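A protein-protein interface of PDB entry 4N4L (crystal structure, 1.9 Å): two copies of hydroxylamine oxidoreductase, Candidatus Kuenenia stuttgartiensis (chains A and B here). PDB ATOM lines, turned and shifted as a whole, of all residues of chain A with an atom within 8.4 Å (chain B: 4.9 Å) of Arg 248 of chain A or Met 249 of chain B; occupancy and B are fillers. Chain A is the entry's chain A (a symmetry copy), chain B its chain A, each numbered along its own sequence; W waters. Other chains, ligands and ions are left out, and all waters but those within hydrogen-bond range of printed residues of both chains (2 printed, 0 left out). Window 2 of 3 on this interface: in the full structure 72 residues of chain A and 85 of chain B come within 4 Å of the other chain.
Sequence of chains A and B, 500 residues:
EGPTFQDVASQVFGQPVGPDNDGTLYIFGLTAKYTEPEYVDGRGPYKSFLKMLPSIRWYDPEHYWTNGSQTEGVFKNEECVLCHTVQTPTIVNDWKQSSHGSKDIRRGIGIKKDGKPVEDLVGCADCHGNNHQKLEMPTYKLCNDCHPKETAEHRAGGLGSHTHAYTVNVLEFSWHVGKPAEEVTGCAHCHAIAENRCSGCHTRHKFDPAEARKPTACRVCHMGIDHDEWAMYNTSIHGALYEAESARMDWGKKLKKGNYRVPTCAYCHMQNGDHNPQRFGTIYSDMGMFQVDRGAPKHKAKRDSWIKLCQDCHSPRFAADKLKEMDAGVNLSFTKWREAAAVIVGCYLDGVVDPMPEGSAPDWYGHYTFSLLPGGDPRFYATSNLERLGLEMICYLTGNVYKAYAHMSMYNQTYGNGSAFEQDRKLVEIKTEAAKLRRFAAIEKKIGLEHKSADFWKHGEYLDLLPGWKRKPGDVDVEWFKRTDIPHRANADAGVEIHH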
ATOM      1  N   TYR A 242     -24.343  23.578  25.629  1.00  0.00           N
ATOM      2  CA  TYR A 242     -23.986  22.632  24.567  1.00  0.00           C
ATOM      3  C   TYR A 242     -23.784  21.234  25.153  1.00  0.00           C
ATOM      4  O   TYR A 242     -24.352  20.259  24.657  1.00  0.00           O
ATOM      5  CB  TYR A 242     -22.725  23.072  23.812  1.00  0.00           C
ATOM      6  CG  TYR A 242     -21.937  21.906  23.266  1.00  0.00           C
ATOM      7  CD1 TYR A 242     -22.431  21.139  22.213  1.00  0.00           C
ATOM      8  CD2 TYR A 242     -20.714  21.548  23.823  1.00  0.00           C
ATOM      9  CE1 TYR A 242     -21.714  20.047  21.719  1.00  0.00           C
ATOM     10  CE2 TYR A 242     -19.990  20.465  23.337  1.00  0.00           C
ATOM     11  CZ  TYR A 242     -20.493  19.722  22.288  1.00  0.00           C
ATOM     12  OH  TYR A 242     -19.784  18.645  21.811  1.00  0.00           O
ATOM     13  N   GLU A 243     -22.997  21.138  26.221  1.00  0.00           N
ATOM     14  CA  GLU A 243     -22.715  19.841  26.837  1.00  0.00           C
ATOM     15  C   GLU A 243     -23.991  19.206  27.381  1.00  0.00           C
ATOM     16  O   GLU A 243     -24.207  17.996  27.235  1.00  0.00           O
ATOM     17  CB  GLU A 243     -21.661  19.980  27.939  1.00  0.00           C
ATOM     18  CG  GLU A 243     -21.284  18.655  28.609  1.00  0.00           C
ATOM     19  CD  GLU A 243     -20.230  18.809  29.697  1.00  0.00           C
ATOM     20  OE1 GLU A 243     -19.463  19.799  29.673  1.00  0.00           O
ATOM     21  OE2 GLU A 243     -20.175  17.924  30.580  1.00  0.00           O
ATOM     22  N   ALA A 244     -24.841  20.030  27.991  1.00  0.00           N
ATOM     23  CA  ALA A 244     -26.108  19.563  28.541  1.00  0.00           C
ATOM     24  C   ALA A 244     -27.071  19.040  27.470  1.00  0.00           C
ATOM     25  O   ALA A 244     -27.717  18.011  27.668  1.00  0.00           O
ATOM     26  CB  ALA A 244     -26.778  20.684  29.345  1.00  0.00           C
ATOM     27  N   GLU A 245     -27.167  19.749  26.347  1.00  0.00           N
ATOM     28  CA  GLU A 245     -28.194  19.476  25.334  1.00  0.00           C
ATOM     29  C   GLU A 245     -27.727  18.672  24.118  1.00  0.00           C
ATOM     30  O   GLU A 245     -28.557  18.240  23.309  1.00  0.00           O
ATOM     31  CB  GLU A 245     -28.829  20.797  24.870  1.00  0.00           C
ATOM     32  CG  GLU A 245     -29.443  21.579  26.024  1.00  0.00           C
ATOM     33  CD  GLU A 245     -30.466  22.624  25.611  1.00  0.00           C
ATOM     34  OE1 GLU A 245     -31.069  23.210  26.534  1.00  0.00           O
ATOM     35  OE2 GLU A 245     -30.678  22.864  24.396  1.00  0.00           O
ATOM     36  N   SER A 246     -26.423  18.435  23.992  1.00  0.00           N
ATOM     37  CA  SER A 246     -25.891  17.804  22.784  1.00  0.00           C
ATOM     38  C   SER A 246     -26.519  16.451  22.477  1.00  0.00           C
ATOM     39  O   SER A 246     -26.785  16.145  21.315  1.00  0.00           O
ATOM     40  CB  SER A 246     -24.377  17.618  22.858  1.00  0.00           C
ATOM     41  OG  SER A 246     -23.916  17.104  21.618  1.00  0.00           O
ATOM     42  N   ALA A 247     -26.746  15.650  23.514  1.00  0.00           N
ATOM     43  CA  ALA A 247     -27.200  14.273  23.342  1.00  0.00           C
ATOM     44  C   ALA A 247     -28.622  14.170  22.801  1.00  0.00           C
ATOM     45  O   ALA A 247     -28.962  13.184  22.139  1.00  0.00           O
ATOM     46  CB  ALA A 247     -27.096  13.511  24.665  1.00  0.00           C
ATOM     47  N   ARG A 248     -29.449  15.169  23.089  1.00  0.00           N
ATOM     48  CA  ARG A 248     -30.878  15.092  22.766  1.00  0.00           C
ATOM     49  C   ARG A 248     -31.370  16.153  21.780  1.00  0.00           C
ATOM     50  O   ARG A 248     -32.485  16.047  21.263  1.00  0.00           O
ATOM     51  CB  ARG A 248     -31.680  15.126  24.059  1.00  0.00           C
ATOM     52  CG  ARG A 248     -31.394  13.910  24.942  1.00  0.00           C
ATOM     53  CD  ARG A 248     -32.009  14.026  26.326  1.00  0.00           C
ATOM     54  NE  ARG A 248     -31.608  12.910  27.186  1.00  0.00           N
ATOM     55  CZ  ARG A 248     -30.427  12.804  27.807  1.00  0.00           C
ATOM     56  NH1 ARG A 248     -29.488  13.744  27.675  1.00  0.00           N
ATOM     57  NH2 ARG A 248     -30.181  11.743  28.568  1.00  0.00           N
ATOM     58  N   MET A 249     -30.546  17.160  21.502  1.00  0.00           N
ATOM     59  CA  MET A 249     -30.936  18.211  20.565  1.00  0.00           C
ATOM     60  C   MET A 249     -30.875  17.729  19.113  1.00  0.00           C
ATOM     61  O   MET A 249     -30.180  16.756  18.777  1.00  0.00           O
ATOM     62  CB  MET A 249     -30.083  19.472  20.760  1.00  0.00           C
ATOM     63  CG  MET A 249     -28.608  19.308  20.440  1.00  0.00           C
ATOM     64  SD  MET A 249     -27.649  20.726  21.008  1.00  0.00           S
ATOM     65  CE  MET A 249     -27.750  21.763  19.542  1.00  0.00           C
ATOM     66  N   ASP A 250     -31.612  18.420  18.256  1.00  0.00           N
ATOM     67  CA  ASP A 250     -31.694  18.063  16.856  1.00  0.00           C
ATOM     68  C   ASP A 250     -30.607  18.798  16.086  1.00  0.00           C
ATOM     69  O   ASP A 250     -30.741  19.989  15.778  1.00  0.00           O
ATOM     70  CB  ASP A 250     -33.081  18.406  16.305  1.00  0.00           C
ATOM     71  CG  ASP A 250     -33.268  17.963  14.868  1.00  0.00           C
ATOM     72  OD1 ASP A 250     -34.377  18.173  14.348  1.00  0.00           O
ATOM     73  OD2 ASP A 250     -32.326  17.405  14.263  1.00  0.00           O
ATOM     74  N   TRP A 251     -29.536  18.070  15.777  1.00  0.00           N
ATOM     75  CA  TRP A 251     -28.398  18.612  15.036  1.00  0.00           C
ATOM     76  C   TRP A 251     -28.623  18.596  13.522  1.00  0.00           C
ATOM     77  O   TRP A 251     -27.776  19.070  12.766  1.00  0.00           O
ATOM     78  CB  TRP A 251     -27.137  17.807  15.345  1.00  0.00           C
ATOM     79  CG  TRP A 251     -26.602  18.005  16.725  1.00  0.00           C
ATOM     80  CD1 TRP A 251     -26.708  17.147  17.773  1.00  0.00           C
ATOM     81  CD2 TRP A 251     -25.851  19.127  17.195  1.00  0.00           C
ATOM     82  NE1 TRP A 251     -26.070  17.665  18.880  1.00  0.00           N
ATOM     83  CE2 TRP A 251     -25.539  18.884  18.551  1.00  0.00           C
ATOM     84  CE3 TRP A 251     -25.415  20.321  16.604  1.00  0.00           C
ATOM     85  CZ2 TRP A 251     -24.804  19.785  19.323  1.00  0.00           C
ATOM     86  CZ3 TRP A 251     -24.694  21.220  17.375  1.00  0.00           C
ATOM     87  CH2 TRP A 251     -24.398  20.947  18.724  1.00  0.00           C
ATOM     88  N   LYS B 214     -27.567  18.501  36.110  1.00  0.00           N
ATOM     89  CA  LYS B 214     -26.321  18.143  35.426  1.00  0.00           C
ATOM     90  C   LYS B 214     -25.145  18.978  35.952  1.00  0.00           C
ATOM     91  O   LYS B 214     -25.345  20.106  36.389  1.00  0.00           O
ATOM     92  CB  LYS B 214     -26.484  18.342  33.921  1.00  0.00           C
ATOM     93  CG  LYS B 214     -27.666  17.580  33.338  1.00  0.00           C
ATOM     94  CD  LYS B 214     -27.756  17.694  31.824  1.00  0.00           C
ATOM     95  CE  LYS B 214     -29.033  17.012  31.324  1.00  0.00           C
ATOM     96  NZ  LYS B 214     -29.172  16.920  29.834  1.00  0.00           N
ATOM     97  N   GLU B 245     -22.645   8.045  30.981  1.00  0.00           N
ATOM     98  CA  GLU B 245     -24.085   7.794  31.104  1.00  0.00           C
ATOM     99  C   GLU B 245     -24.993   8.987  30.796  1.00  0.00           C
ATOM    100  O   GLU B 245     -26.215   8.822  30.695  1.00  0.00           O
ATOM    101  CB  GLU B 245     -24.400   7.249  32.506  1.00  0.00           C
ATOM    102  CG  GLU B 245     -23.629   5.972  32.816  1.00  0.00           C
ATOM    103  CD  GLU B 245     -24.209   5.138  33.945  1.00  0.00           C
ATOM    104  OE1 GLU B 245     -23.669   4.032  34.157  1.00  0.00           O
ATOM    105  OE2 GLU B 245     -25.186   5.560  34.614  1.00  0.00           O
ATOM    106  N   SER B 246     -24.420  10.175  30.615  1.00  0.00           N
ATOM    107  CA  SER B 246     -25.232  11.383  30.466  1.00  0.00           C
ATOM    108  C   SER B 246     -26.236  11.304  29.322  1.00  0.00           C
ATOM    109  O   SER B 246     -27.368  11.765  29.463  1.00  0.00           O
ATOM    110  CB  SER B 246     -24.371  12.626  30.256  1.00  0.00           C
ATOM    111  OG  SER B 246     -25.213  13.768  30.228  1.00  0.00           O
ATOM    112  N   ALA B 247     -25.815  10.730  28.199  1.00  0.00           N
ATOM    113  CA  ALA B 247     -26.623  10.727  26.983  1.00  0.00           C
ATOM    114  C   ALA B 247     -27.877   9.866  27.093  1.00  0.00           C
ATOM    115  O   ALA B 247     -28.876  10.139  26.420  1.00  0.00           O
ATOM    116  CB  ALA B 247     -25.784  10.265  25.789  1.00  0.00           C
ATOM    117  N   ARG B 248     -27.824   8.829  27.922  1.00  0.00           N
ATOM    118  CA  ARG B 248     -28.907   7.842  27.978  1.00  0.00           C
ATOM    119  C   ARG B 248     -29.618   7.744  29.328  1.00  0.00           C
ATOM    120  O   ARG B 248     -30.680   7.125  29.425  1.00  0.00           O
ATOM    121  CB  ARG B 248     -28.364   6.488  27.541  1.00  0.00           C
ATOM    122  CG  ARG B 248     -27.896   6.502  26.085  1.00  0.00           C
ATOM    123  CD  ARG B 248     -27.153   5.237  25.691  1.00  0.00           C
ATOM    124  NE  ARG B 248     -26.606   5.336  24.335  1.00  0.00           N
ATOM    125  CZ  ARG B 248     -25.492   6.000  24.002  1.00  0.00           C
ATOM    126  NH1 ARG B 248     -24.774   6.651  24.920  1.00  0.00           N
ATOM    127  NH2 ARG B 248     -25.092   6.014  22.736  1.00  0.00           N
ATOM    128  N   MET B 249     -29.056   8.365  30.362  1.00  0.00           N
ATOM    129  CA  MET B 249     -29.674   8.329  31.685  1.00  0.00           C
ATOM    130  C   MET B 249     -30.896   9.249  31.766  1.00  0.00           C
ATOM    131  O   MET B 249     -31.053  10.196  30.980  1.00  0.00           O
ATOM    132  CB  MET B 249     -28.658   8.670  32.783  1.00  0.00           C
ATOM    133  CG  MET B 249     -28.113  10.087  32.739  1.00  0.00           C
ATOM    134  SD  MET B 249     -26.702  10.286  33.844  1.00  0.00           S
ATOM    135  CE  MET B 249     -27.566  10.771  35.346  1.00  0.00           C
ATOM    136  N   ASP B 250     -31.760   8.957  32.728  1.00  0.00           N
ATOM    137  CA  ASP B 250     -32.985   9.706  32.907  1.00  0.00           C
ATOM    138  C   ASP B 250     -32.733  10.860  33.867  1.00  0.00           C
ATOM    139  O   ASP B 250     -32.682  10.672  35.088  1.00  0.00           O
ATOM    140  CB  ASP B 250     -34.091   8.788  33.436  1.00  0.00           C
ATOM    141  CG  ASP B 250     -35.430   9.487  33.550  1.00  0.00           C
ATOM    142  OD1 ASP B 250     -36.395   8.809  33.943  1.00  0.00           O
ATOM    143  OD2 ASP B 250     -35.527  10.697  33.247  1.00  0.00           O
ATOM    144  N   TRP B 251     -32.581  12.052  33.296  1.00  0.00           N
ATOM    145  CA  TRP B 251     -32.335  13.272  34.064  1.00  0.00           C
ATOM    146  C   TRP B 251     -33.625  13.895  34.604  1.00  0.00           C
ATOM    147  O   TRP B 251     -33.578  14.897  35.316  1.00  0.00           O
ATOM    148  CB  TRP B 251     -31.626  14.308  33.195  1.00  0.00           C
ATOM    149  CG  TRP B 251     -30.207  13.975  32.871  1.00  0.00           C
ATOM    150  CD1 TRP B 251     -29.727  13.506  31.689  1.00  0.00           C
ATOM    151  CD2 TRP B 251     -29.080  14.116  33.739  1.00  0.00           C
ATOM    152  NE1 TRP B 251     -28.361  13.337  31.764  1.00  0.00           N
ATOM    153  CE2 TRP B 251     -27.940  13.701  33.015  1.00  0.00           C
ATOM    154  CE3 TRP B 251     -28.921  14.545  35.064  1.00  0.00           C
ATOM    155  CZ2 TRP B 251     -26.658  13.712  33.567  1.00  0.00           C
ATOM    156  CZ3 TRP B 251     -27.649  14.546  35.615  1.00  0.00           C
ATOM    157  CH2 TRP B 251     -26.532  14.129  34.866  1.00  0.00           C
ATOM    158  N   TYR B 260     -30.624   7.763  40.972  1.00  0.00           N
ATOM    159  CA  TYR B 260     -29.418   7.952  40.162  1.00  0.00           C
ATOM    160  C   TYR B 260     -28.345   6.927  40.477  1.00  0.00           C
ATOM    161  O   TYR B 260     -28.121   6.589  41.637  1.00  0.00           O
ATOM    162  CB  TYR B 260     -28.853   9.370  40.362  1.00  0.00           C
ATOM    163  CG  TYR B 260     -29.692  10.401  39.662  1.00  0.00           C
ATOM    164  CD1 TYR B 260     -29.453  10.726  38.333  1.00  0.00           C
ATOM    165  CD2 TYR B 260     -30.771  11.002  40.303  1.00  0.00           C
ATOM    166  CE1 TYR B 260     -30.244  11.641  37.668  1.00  0.00           C
ATOM    167  CE2 TYR B 260     -31.573  11.916  39.643  1.00  0.00           C
ATOM    168  CZ  TYR B 260     -31.304  12.231  38.325  1.00  0.00           C
ATOM    169  OH  TYR B 260     -32.096  13.132  37.652  1.00  0.00           O
ATOM    170  N   VAL B 262     -25.163   7.619  39.033  1.00  0.00           N
ATOM    171  CA  VAL B 262     -24.030   8.532  39.058  1.00  0.00           C
ATOM    172  C   VAL B 262     -24.420   9.803  39.803  1.00  0.00           C
ATOM    173  O   VAL B 262     -25.404  10.451  39.434  1.00  0.00           O
ATOM    174  CB  VAL B 262     -23.604   8.916  37.629  1.00  0.00           C
ATOM    175  CG1 VAL B 262     -22.442   9.928  37.654  1.00  0.00           C
ATOM    176  CG2 VAL B 262     -23.225   7.668  36.840  1.00  0.00           C
HETATM  177  O   HOH W   1     -27.233  15.023  28.814  1.00  0.00           O
HETATM  178  O   HOH W   2     -24.253  16.101  29.650  1.00  0.00           O
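Arg 248 of chain A touches just these residues of chain B: Lys 214 (3.9 Å), Ser 246 (3.0 Å), Ala 247 (3.0 Å), Arg 248 (3.8 Å), Met 249 (3.0 Å) and Trp 251 (3.6 Å).
Met 249 of chain B touches one residue of chain A.
Of the printed residues of chain A, Ser 246 of chain B touches Arg 248 (3.0 Å).
Of the printed residues of chain A, Arg 248 of chain B touches Arg 248.
Printed residues of chain A within 4 Å of Ala 247 of chain B: Ala 247 (3.7 Å) and Arg 248 (3.0 Å).
Of the printed residues of chain A, Lys 214 of chain B touches Ala 244 (2.8 Å) and Arg 248 (3.9 Å).
Printed residues of chain A within 4 Å of Trp 251 of chain B: Arg 248 (3.6 Å).
The nearest printed residue of chain B that does not touch Arg 248 of chain A is Asp 250 of chain B (5.2 Å).
The nearest residue of chain A that does not touch Met 249 of chain B is Ala 247 of chain A (7.9 Å).
The nearest printed residue of chain A that does not touch Ala 247 of chain B is Ser 246 of chain A (7.1 Å).
Water W2 bridges the side-chain hydroxyl (OG) of Ser 246 of chain B (2.6 Å) and the backbone carbonyl oxygen (O) of Glu 243 of chain A (3.1 Å).
Water W1 lies within hydrogen-bond range of the side-chain hydroxyl of Ser 246 of chain B (2.8 Å), the guanidinium group of Arg 248 of chain A (2.8 Å), the side-chain amino group of Lys 214 of chain B (2.9 Å) and the backbone carbonyl oxygen of Ala 244 of chain A (3.2 Å).
Among the printed residues, merely in contact across the chains: Arg 248 of chain A with Trp 251 of chain B (3.6 Å), Ala 247 of chain A with Ala 247 of chain B (3.7 Å), Arg 248 of chain A with Arg 248 of chain B (3.8 Å) and Arg 248 of chain A with Lys 214 of chain B (3.9 Å).
The backbone carbonyl oxygen (O) of Ala 244 of chain A sits at hydrogen-bond distance from the side-chain amino group (NZ) of Lys 214 of chain B, at 2.8 Å.
NH2 of Arg 248 of chain A sits at hydrogen-bond distance from O of Met 249 of chain B (3.0 Å).
The backbone carbonyl oxygen of Ser 246 of chain B sits at hydrogen-bond distance from the guanidinium group of Arg 248 of chain A (3.0 Å).
The backbone carbonyl oxygen of Ala 247 of chain B lies within hydrogen-bond range of the guanidinium group of Arg 248 of chain A, at 3.0 Å.
O of Trp 251 of chain B sits at hydrogen-bond distance from OH of Tyr 260 of chain B, at 3.3 Å.
The backbone carbonyl oxygen of Ser 246 of chain B is in hydrogen-bond range of the indole nitrogen of Trp 251 of chain B (3.0 Å).
Of the 10 printed residues of chain B, 6 touch a printed residue of chain A.
Of the 10 printed residues of chain A, 3 touch a printed residue of chain B.
Printed residues of chain A that touch a printed residue of chain B: Ala 244, Ala 247 and Arg 248.
Hydrophobic or aromatic side chains of chain A that line the printed part of chain B: Ala 247.
Among the printed residues, no Asp or Glu carboxylate lies within 4 Å of a Lys or Arg side-chain nitrogen of the other chain.
Ala 247 of chain B touches its own counterpart, Ala 247 of chain A.
Arg 248 of chain A touches Ala 247 of chain B, but with the chains exchanged Ala 247 of chain A does not touch Arg 248 of chain B (5.7 Å).
Arg 248 of chain B touches its own counterpart, Arg 248 of chain A.
Arg 248 of chain A touches Met 249 of chain B, but with the chains exchanged Met 249 of chain A does not touch Arg 248 of chain B (10.9 Å).
Positions printed for both chains: 245, 246, 247, 248, 249, 250 and 251.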
